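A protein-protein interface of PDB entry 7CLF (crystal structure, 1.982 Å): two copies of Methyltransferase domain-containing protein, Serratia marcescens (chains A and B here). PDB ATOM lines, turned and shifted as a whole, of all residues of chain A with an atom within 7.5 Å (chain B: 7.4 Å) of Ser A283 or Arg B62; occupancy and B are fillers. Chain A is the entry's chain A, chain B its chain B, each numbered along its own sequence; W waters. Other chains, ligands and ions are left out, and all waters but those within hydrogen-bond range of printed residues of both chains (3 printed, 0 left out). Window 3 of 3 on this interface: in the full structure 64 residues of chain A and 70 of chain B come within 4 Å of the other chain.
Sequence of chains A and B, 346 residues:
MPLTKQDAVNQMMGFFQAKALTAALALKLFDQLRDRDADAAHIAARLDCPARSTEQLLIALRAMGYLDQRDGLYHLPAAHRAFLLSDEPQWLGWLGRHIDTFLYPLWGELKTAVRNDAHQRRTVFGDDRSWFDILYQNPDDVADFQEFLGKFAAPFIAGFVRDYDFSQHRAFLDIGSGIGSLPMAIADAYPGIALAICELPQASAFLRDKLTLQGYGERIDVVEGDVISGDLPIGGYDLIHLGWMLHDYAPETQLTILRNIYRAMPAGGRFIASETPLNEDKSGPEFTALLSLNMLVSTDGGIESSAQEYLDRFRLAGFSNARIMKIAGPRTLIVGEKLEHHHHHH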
ATOM      1  N   LEU A 278     -13.228   9.171 -17.242  1.00  0.00           N
ATOM      2  CA  LEU A 278     -13.756   8.685 -18.508  1.00  0.00           C
ATOM      3  C   LEU A 278     -15.269   8.503 -18.393  1.00  0.00           C
ATOM      4  O   LEU A 278     -15.817   8.330 -17.297  1.00  0.00           O
ATOM      5  CB  LEU A 278     -13.095   7.364 -18.903  1.00  0.00           C
ATOM      6  CG  LEU A 278     -11.591   7.404 -19.159  1.00  0.00           C
ATOM      7  CD1 LEU A 278     -11.074   5.988 -19.115  1.00  0.00           C
ATOM      8  CD2 LEU A 278     -11.293   8.047 -20.509  1.00  0.00           C
ATOM      9  N   ASN A 279     -15.952   8.556 -19.541  1.00  0.00           N
ATOM     10  CA  ASN A 279     -17.396   8.386 -19.518  1.00  0.00           C
ATOM     11  C   ASN A 279     -17.762   6.943 -19.152  1.00  0.00           C
ATOM     12  O   ASN A 279     -16.911   6.047 -19.075  1.00  0.00           O
ATOM     13  CB  ASN A 279     -18.023   8.822 -20.848  1.00  0.00           C
ATOM     14  CG  ASN A 279     -17.378   8.169 -22.057  1.00  0.00           C
ATOM     15  OD1 ASN A 279     -16.720   7.139 -21.945  1.00  0.00           O
ATOM     16  ND2 ASN A 279     -17.569   8.773 -23.230  1.00  0.00           N
ATOM     17  N   GLU A 280     -19.060   6.739 -18.892  1.00  0.00           N
ATOM     18  CA  GLU A 280     -19.543   5.469 -18.360  1.00  0.00           C
ATOM     19  C   GLU A 280     -19.092   4.282 -19.207  1.00  0.00           C
ATOM     20  O   GLU A 280     -18.678   3.252 -18.668  1.00  0.00           O
ATOM     21  CB  GLU A 280     -21.066   5.511 -18.250  1.00  0.00           C
ATOM     22  CG  GLU A 280     -21.731   4.152 -18.102  1.00  0.00           C
ATOM     23  CD  GLU A 280     -23.227   4.215 -18.373  1.00  0.00           C
ATOM     24  OE1 GLU A 280     -23.952   3.281 -17.957  1.00  0.00           O
ATOM     25  OE2 GLU A 280     -23.673   5.204 -19.003  1.00  0.00           O
ATOM     26  N   ASP A 281     -19.149   4.405 -20.531  1.00  0.00           N
ATOM     27  CA  ASP A 281     -18.741   3.316 -21.406  1.00  0.00           C
ATOM     28  C   ASP A 281     -17.285   3.438 -21.863  1.00  0.00           C
ATOM     29  O   ASP A 281     -16.897   2.803 -22.847  1.00  0.00           O
ATOM     30  CB  ASP A 281     -19.696   3.214 -22.597  1.00  0.00           C
ATOM     31  CG  ASP A 281     -19.373   4.193 -23.706  1.00  0.00           C
ATOM     32  OD1 ASP A 281     -19.041   5.365 -23.411  1.00  0.00           O
ATOM     33  OD2 ASP A 281     -19.457   3.778 -24.886  1.00  0.00           O
ATOM     34  N   LYS A 282     -16.475   4.219 -21.150  1.00  0.00           N
ATOM     35  CA  LYS A 282     -15.033   4.358 -21.389  1.00  0.00           C
ATOM     36  C   LYS A 282     -14.708   4.456 -22.879  1.00  0.00           C
ATOM     37  O   LYS A 282     -13.826   3.771 -23.405  1.00  0.00           O
ATOM     38  CB  LYS A 282     -14.258   3.220 -20.715  1.00  0.00           C
ATOM     39  CG  LYS A 282     -14.246   3.338 -19.186  1.00  0.00           C
ATOM     40  CD  LYS A 282     -13.607   2.117 -18.521  1.00  0.00           C
ATOM     41  CE  LYS A 282     -12.455   2.491 -17.601  1.00  0.00           C
ATOM     42  NZ  LYS A 282     -11.675   1.276 -17.206  1.00  0.00           N
ATOM     43  N   SER A 283     -15.439   5.345 -23.551  1.00  0.00           N
ATOM     44  CA  SER A 283     -15.265   5.679 -24.956  1.00  0.00           C
ATOM     45  C   SER A 283     -14.761   7.101 -25.156  1.00  0.00           C
ATOM     46  O   SER A 283     -14.782   7.610 -26.282  1.00  0.00           O
ATOM     47  CB  SER A 283     -16.593   5.517 -25.688  1.00  0.00           C
ATOM     48  OG  SER A 283     -17.478   6.562 -25.301  1.00  0.00           O
ATOM     49  N   GLY A 284     -14.336   7.766 -24.091  1.00  0.00           N
ATOM     50  CA  GLY A 284     -13.963   9.157 -24.166  1.00  0.00           C
ATOM     51  C   GLY A 284     -14.120   9.819 -22.810  1.00  0.00           C
ATOM     52  O   GLY A 284     -14.257   9.139 -21.788  1.00  0.00           O
ATOM     53  N   PRO A 285     -14.082  11.159 -22.762  1.00  0.00           N
ATOM     54  CA  PRO A 285     -13.859  12.079 -23.885  1.00  0.00           C
ATOM     55  C   PRO A 285     -12.416  12.011 -24.364  1.00  0.00           C
ATOM     56  O   PRO A 285     -11.561  11.461 -23.660  1.00  0.00           O
ATOM     57  CB  PRO A 285     -14.168  13.459 -23.300  1.00  0.00           C
ATOM     58  CG  PRO A 285     -14.575  13.236 -21.879  1.00  0.00           C
ATOM     59  CD  PRO A 285     -14.137  11.868 -21.473  1.00  0.00           C
ATOM     60  N   GLU A 286     -12.161  12.579 -25.541  1.00  0.00           N
ATOM     61  CA  GLU A 286     -10.892  12.350 -26.221  1.00  0.00           C
ATOM     62  C   GLU A 286      -9.720  12.930 -25.441  1.00  0.00           C
ATOM     63  O   GLU A 286      -8.661  12.296 -25.345  1.00  0.00           O
ATOM     64  CB  GLU A 286     -10.945  12.931 -27.631  1.00  0.00           C
ATOM     65  CG  GLU A 286      -9.588  13.099 -28.298  1.00  0.00           C
ATOM     66  CD  GLU A 286      -9.705  13.614 -29.729  1.00  0.00           C
ATOM     67  OE1 GLU A 286     -10.812  13.534 -30.293  1.00  0.00           O
ATOM     68  OE2 GLU A 286      -8.693  14.085 -30.289  1.00  0.00           O
ATOM     69  N   ALA A 289      -9.025  10.568 -22.498  1.00  0.00           N
ATOM     70  CA  ALA A 289      -8.389   9.350 -22.994  1.00  0.00           C
ATOM     71  C   ALA A 289      -6.921   9.583 -23.317  1.00  0.00           C
ATOM     72  O   ALA A 289      -6.073   8.725 -23.043  1.00  0.00           O
ATOM     73  CB  ALA A 289      -9.129   8.828 -24.239  1.00  0.00           C
ATOM     74  N   GLN B  56      -5.660   1.354 -22.593  1.00  0.00           N
ATOM     75  CA  GLN B  56      -5.482   2.803 -22.575  1.00  0.00           C
ATOM     76  C   GLN B  56      -5.294   3.337 -23.986  1.00  0.00           C
ATOM     77  O   GLN B  56      -5.850   4.381 -24.356  1.00  0.00           O
ATOM     78  CB  GLN B  56      -4.279   3.184 -21.710  1.00  0.00           C
ATOM     79  CG  GLN B  56      -4.551   3.225 -20.222  1.00  0.00           C
ATOM     80  CD  GLN B  56      -3.296   3.490 -19.426  1.00  0.00           C
ATOM     81  OE1 GLN B  56      -2.459   2.601 -19.239  1.00  0.00           O
ATOM     82  NE2 GLN B  56      -3.147   4.723 -18.959  1.00  0.00           N
ATOM     83  N   LEU B  57      -4.498   2.636 -24.791  1.00  0.00           N
ATOM     84  CA  LEU B  57      -4.309   3.075 -26.168  1.00  0.00           C
ATOM     85  C   LEU B  57      -5.583   2.883 -26.976  1.00  0.00           C
ATOM     86  O   LEU B  57      -5.956   3.752 -27.774  1.00  0.00           O
ATOM     87  CB  LEU B  57      -3.134   2.326 -26.799  1.00  0.00           C
ATOM     88  CG  LEU B  57      -2.768   2.681 -28.246  1.00  0.00           C
ATOM     89  CD1 LEU B  57      -2.508   4.162 -28.374  1.00  0.00           C
ATOM     90  CD2 LEU B  57      -1.537   1.889 -28.691  1.00  0.00           C
ATOM     91  N   LEU B  58      -6.279   1.763 -26.766  1.00  0.00           N
ATOM     92  CA  LEU B  58      -7.501   1.511 -27.520  1.00  0.00           C
ATOM     93  C   LEU B  58      -8.569   2.559 -27.219  1.00  0.00           C
ATOM     94  O   LEU B  58      -9.264   3.020 -28.127  1.00  0.00           O
ATOM     95  CB  LEU B  58      -8.019   0.105 -27.227  1.00  0.00           C
ATOM     96  CG  LEU B  58      -7.203  -1.014 -27.874  1.00  0.00           C
ATOM     97  CD1 LEU B  58      -7.409  -2.318 -27.131  1.00  0.00           C
ATOM     98  CD2 LEU B  58      -7.612  -1.129 -29.337  1.00  0.00           C
ATOM     99  N   ILE B  59      -8.710   2.953 -25.953  1.00  0.00           N
ATOM    100  CA  ILE B  59      -9.691   3.985 -25.620  1.00  0.00           C
ATOM    101  C   ILE B  59      -9.352   5.286 -26.328  1.00  0.00           C
ATOM    102  O   ILE B  59     -10.224   5.939 -26.910  1.00  0.00           O
ATOM    103  CB  ILE B  59      -9.780   4.171 -24.094  1.00  0.00           C
ATOM    104  CG1 ILE B  59     -10.544   3.008 -23.467  1.00  0.00           C
ATOM    105  CG2 ILE B  59     -10.463   5.498 -23.744  1.00  0.00           C
ATOM    106  CD1 ILE B  59     -10.177   2.758 -22.012  1.00  0.00           C
ATOM    107  N   ALA B  60      -8.074   5.660 -26.331  1.00  0.00           N
ATOM    108  CA  ALA B  60      -7.657   6.883 -27.013  1.00  0.00           C
ATOM    109  C   ALA B  60      -7.982   6.825 -28.508  1.00  0.00           C
ATOM    110  O   ALA B  60      -8.534   7.777 -29.076  1.00  0.00           O
ATOM    111  CB  ALA B  60      -6.163   7.112 -26.781  1.00  0.00           C
ATOM    112  N   LEU B  61      -7.667   5.693 -29.156  1.00  0.00           N
ATOM    113  CA  LEU B  61      -7.988   5.526 -30.573  1.00  0.00           C
ATOM    114  C   LEU B  61      -9.489   5.559 -30.814  1.00  0.00           C
ATOM    115  O   LEU B  61      -9.950   6.061 -31.848  1.00  0.00           O
ATOM    116  CB  LEU B  61      -7.397   4.212 -31.089  1.00  0.00           C
ATOM    117  CG  LEU B  61      -5.875   4.158 -31.042  1.00  0.00           C
ATOM    118  CD1 LEU B  61      -5.349   2.802 -31.522  1.00  0.00           C
ATOM    119  CD2 LEU B  61      -5.296   5.315 -31.865  1.00  0.00           C
ATOM    120  N   ARG B  62     -10.272   5.009 -29.884  1.00  0.00           N
ATOM    121  CA  ARG B  62     -11.723   5.046 -30.037  1.00  0.00           C
ATOM    122  C   ARG B  62     -12.245   6.465 -29.874  1.00  0.00           C
ATOM    123  O   ARG B  62     -13.077   6.929 -30.663  1.00  0.00           O
ATOM    124  CB  ARG B  62     -12.386   4.099 -29.034  1.00  0.00           C
ATOM    125  CG  ARG B  62     -13.776   4.531 -28.548  1.00  0.00           C
ATOM    126  CD  ARG B  62     -14.815   4.285 -29.609  1.00  0.00           C
ATOM    127  NE  ARG B  62     -16.189   4.416 -29.130  1.00  0.00           N
ATOM    128  CZ  ARG B  62     -16.974   5.458 -29.400  1.00  0.00           C
ATOM    129  NH1 ARG B  62     -16.512   6.473 -30.124  1.00  0.00           N
ATOM    130  NH2 ARG B  62     -18.218   5.497 -28.936  1.00  0.00           N
ATOM    131  N   ALA B  63     -11.745   7.185 -28.873  1.00  0.00           N
ATOM    132  CA  ALA B  63     -12.194   8.562 -28.713  1.00  0.00           C
ATOM    133  C   ALA B  63     -11.699   9.456 -29.844  1.00  0.00           C
ATOM    134  O   ALA B  63     -12.363  10.442 -30.180  1.00  0.00           O
ATOM    135  CB  ALA B  63     -11.753   9.104 -27.352  1.00  0.00           C
ATOM    136  N   MET B  64     -10.539   9.156 -30.434  1.00  0.00           N
ATOM    137  CA  MET B  64     -10.123   9.948 -31.583  1.00  0.00           C
ATOM    138  C   MET B  64     -10.919   9.612 -32.850  1.00  0.00           C
ATOM    139  O   MET B  64     -10.705  10.259 -33.881  1.00  0.00           O
ATOM    140  CB  MET B  64      -8.619   9.798 -31.882  1.00  0.00           C
ATOM    141  CG  MET B  64      -7.591  10.389 -30.843  1.00  0.00           C
ATOM    142  SD  MET B  64      -5.947   9.646 -30.942  1.00  0.00           S
ATOM    143  CE  MET B  64      -5.515  10.245 -32.593  1.00  0.00           C
ATOM    144  N   GLY B  65     -11.807   8.614 -32.814  1.00  0.00           N
ATOM    145  CA  GLY B  65     -12.586   8.246 -33.983  1.00  0.00           C
ATOM    146  C   GLY B  65     -11.935   7.278 -34.954  1.00  0.00           C
ATOM    147  O   GLY B  65     -12.444   7.108 -36.068  1.00  0.00           O
ATOM    148  N   TYR B  66     -10.856   6.615 -34.563  1.00  0.00           N
ATOM    149  CA  TYR B  66     -10.184   5.651 -35.465  1.00  0.00           C
ATOM    150  C   TYR B  66     -10.798   4.261 -35.319  1.00  0.00           C
ATOM    151  O   TYR B  66     -10.739   3.525 -36.253  1.00  0.00           O
ATOM    152  CB  TYR B  66      -8.671   5.665 -35.297  1.00  0.00           C
ATOM    153  CG  TYR B  66      -8.066   6.895 -35.902  1.00  0.00           C
ATOM    154  CD1 TYR B  66      -7.927   8.042 -35.157  1.00  0.00           C
ATOM    155  CD2 TYR B  66      -7.774   6.959 -37.249  1.00  0.00           C
ATOM    156  CE1 TYR B  66      -7.441   9.205 -35.709  1.00  0.00           C
ATOM    157  CE2 TYR B  66      -7.279   8.112 -37.820  1.00  0.00           C
ATOM    158  CZ  TYR B  66      -7.109   9.241 -37.045  1.00  0.00           C
ATOM    159  OH  TYR B  66      -6.630  10.383 -37.582  1.00  0.00           O
ATOM    160  N   LEU B  67     -11.331   3.957 -34.143  1.00  0.00           N
ATOM    161  CA  LEU B  67     -11.991   2.667 -33.848  1.00  0.00           C
ATOM    162  C   LEU B  67     -13.418   2.936 -33.363  1.00  0.00           C
ATOM    163  O   LEU B  67     -13.674   4.000 -32.835  1.00  0.00           O
ATOM    164  CB  LEU B  67     -11.216   1.934 -32.750  1.00  0.00           C
ATOM    165  CG  LEU B  67      -9.754   1.583 -33.021  1.00  0.00           C
ATOM    166  CD1 LEU B  67      -9.158   0.741 -31.914  1.00  0.00           C
ATOM    167  CD2 LEU B  67      -9.583   0.888 -34.350  1.00  0.00           C
ATOM    168  N   ASP B  68     -14.293   1.964 -33.575  1.00  0.00           N
ATOM    169  CA  ASP B  68     -15.690   1.936 -33.064  1.00  0.00           C
ATOM    170  C   ASP B  68     -15.731   0.897 -31.941  1.00  0.00           C
ATOM    171  O   ASP B  68     -14.897  -0.002 -31.967  1.00  0.00           O
ATOM    172  CB  ASP B  68     -16.685   1.440 -34.117  1.00  0.00           C
ATOM    173  CG  ASP B  68     -16.875   2.353 -35.307  1.00  0.00           C
ATOM    174  OD1 ASP B  68     -16.597   3.526 -35.181  1.00  0.00           O
ATOM    175  OD2 ASP B  68     -17.313   1.868 -36.339  1.00  0.00           O
ATOM    176  N   GLN B  69     -16.678   1.051 -31.009  1.00  0.00           N
ATOM    177  CA  GLN B  69     -16.931   0.168 -29.830  1.00  0.00           C
ATOM    178  C   GLN B  69     -17.991   0.802 -28.932  1.00  0.00           C
ATOM    179  O   GLN B  69     -19.164   0.697 -29.262  1.00  0.00           O
ATOM    180  CB  GLN B  69     -15.739   0.039 -28.886  1.00  0.00           C
ATOM    181  CG  GLN B  69     -15.841  -1.177 -27.986  1.00  0.00           C
ATOM    182  CD  GLN B  69     -16.264  -0.829 -26.585  1.00  0.00           C
ATOM    183  OE1 GLN B  69     -15.565  -1.101 -25.633  1.00  0.00           O
ATOM    184  NE2 GLN B  69     -17.401  -0.178 -26.458  1.00  0.00           N
ATOM    185  N   TYR B  74     -13.909  -3.787 -29.941  1.00  0.00           N
ATOM    186  CA  TYR B  74     -13.447  -2.728 -30.870  1.00  0.00           C
ATOM    187  C   TYR B  74     -13.660  -3.194 -32.308  1.00  0.00           C
ATOM    188  O   TYR B  74     -13.453  -4.367 -32.578  1.00  0.00           O
ATOM    189  CB  TYR B  74     -11.991  -2.380 -30.588  1.00  0.00           C
ATOM    190  CG  TYR B  74     -11.821  -1.708 -29.255  1.00  0.00           C
ATOM    191  CD1 TYR B  74     -11.661  -2.443 -28.102  1.00  0.00           C
ATOM    192  CD2 TYR B  74     -11.875  -0.336 -29.143  1.00  0.00           C
ATOM    193  CE1 TYR B  74     -11.519  -1.829 -26.871  1.00  0.00           C
ATOM    194  CE2 TYR B  74     -11.741   0.295 -27.926  1.00  0.00           C
ATOM    195  CZ  TYR B  74     -11.565  -0.453 -26.783  1.00  0.00           C
ATOM    196  OH  TYR B  74     -11.431   0.168 -25.594  1.00  0.00           O
ATOM    197  N   HIS B  75     -14.081  -2.268 -33.163  1.00  0.00           N
ATOM    198  CA  HIS B  75     -14.293  -2.509 -34.609  1.00  0.00           C
ATOM    199  C   HIS B  75     -13.547  -1.464 -35.428  1.00  0.00           C
ATOM    200  O   HIS B  75     -13.683  -0.295 -35.145  1.00  0.00           O
ATOM    201  CB  HIS B  75     -15.771  -2.487 -34.971  1.00  0.00           C
ATOM    202  CG  HIS B  75     -16.019  -2.398 -36.437  1.00  0.00           C
ATOM    203  ND1 HIS B  75     -15.761  -3.423 -37.281  1.00  0.00           N
ATOM    204  CD2 HIS B  75     -16.537  -1.419 -37.194  1.00  0.00           C
ATOM    205  CE1 HIS B  75     -16.082  -3.075 -38.495  1.00  0.00           C
ATOM    206  NE2 HIS B  75     -16.568  -1.868 -38.466  1.00  0.00           N
HETATM  207  O   HOH W   1      -7.073   6.082 -22.628  1.00  0.00           O
HETATM  208  O   HOH W   2     -13.465   2.498 -25.979  1.00  0.00           O
HETATM  209  O   HOH W   3     -18.015   3.284 -27.585  1.00  0.00           O
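OE1 of Glu A286 lies close to O of Ala B63 (3.5 Å).
The side-chain amide oxygen (OD1) of Asn A279 lies within hydrogen-bond range of the backbone NH (N) of Ser A283, at 2.7 Å. The backbone carbonyl oxygen (O) of Gly A284 is in hydrogen-bond range of the backbone NH (N) of Asn A279 (2.9 Å). OD1 of Asp A281 is in hydrogen-bond range of OG of Ser A283, 2.7 Å away. The side-chain amide oxygen of Asn A279 sits at hydrogen-bond distance from the backbone NH of Lys A282, 3.0 Å away.
Among the printed residues, pairs that only touch across the chains: Lys A282 with Ile B59 (3.4 Å), Ser A283 with Arg B62 (3.6 Å), Ser A283 with Ala B63 (3.5 Å), Gly A284 with Ala B63 (3.9 Å), Glu A286 with Met B64 (3.9 Å), Ala A289 with Ile B59 (3.6 Å) and Ala A289 with Ala B60 (3.7 Å).
Of chain A, only Ser A283 (3.6 Å) comes within 4 Å of Arg B62. Printed residues of chain B within 4 Å of Glu A286: Ala B63 and Met B64. Of the printed residues of chain A, Ile B59 touches Lys A282 (3.4 Å) and Ala A289 (3.6 Å). Of the printed residues of chain A, Ala B63 touches Ser A283 (3.5 Å), Gly A284 (3.9 Å) and Glu A286 (3.5 Å). Of the printed residues of chain A, Met B64 touches Glu A286. Of the printed residues of chain B, Lys A282 touches Ile B59 (3.4 Å). The nearest printed residue of chain B that does not touch Lys A282 is Tyr B74 (4.8 Å).
Hydrophobic or aromatic side chains of chain B within 4 Å of the printed part of chain A: Ile B59, Ala B63 and Met B64. Printed residues of chain A that touch a printed residue of chain B: Lys A282, Ser A283, Gly A284, Glu A286 and Ala A289. Among the printed residues, 8 pairs touch across the chains. Among the printed residues, no Asp or Glu carboxylate lies within 4 Å of a Lys or Arg side-chain nitrogen of the other chain.
No position is printed for both chains.
Water W3 lies within hydrogen-bond range of the guanidinium group (NH2) of Arg B62, the side-chain carboxylate (OD2) of Asp A281 and the backbone carbonyl oxygen (O) of Gln B69. Water W1 lies within hydrogen-bond range of the backbone carbonyl oxygen (O) of Gln B56 and the backbone carbonyl oxygen (O) of Ala A289. Water W2 bridges O of Lys A282 (2.9 Å) and OH of Tyr B74 (3.1 Å).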
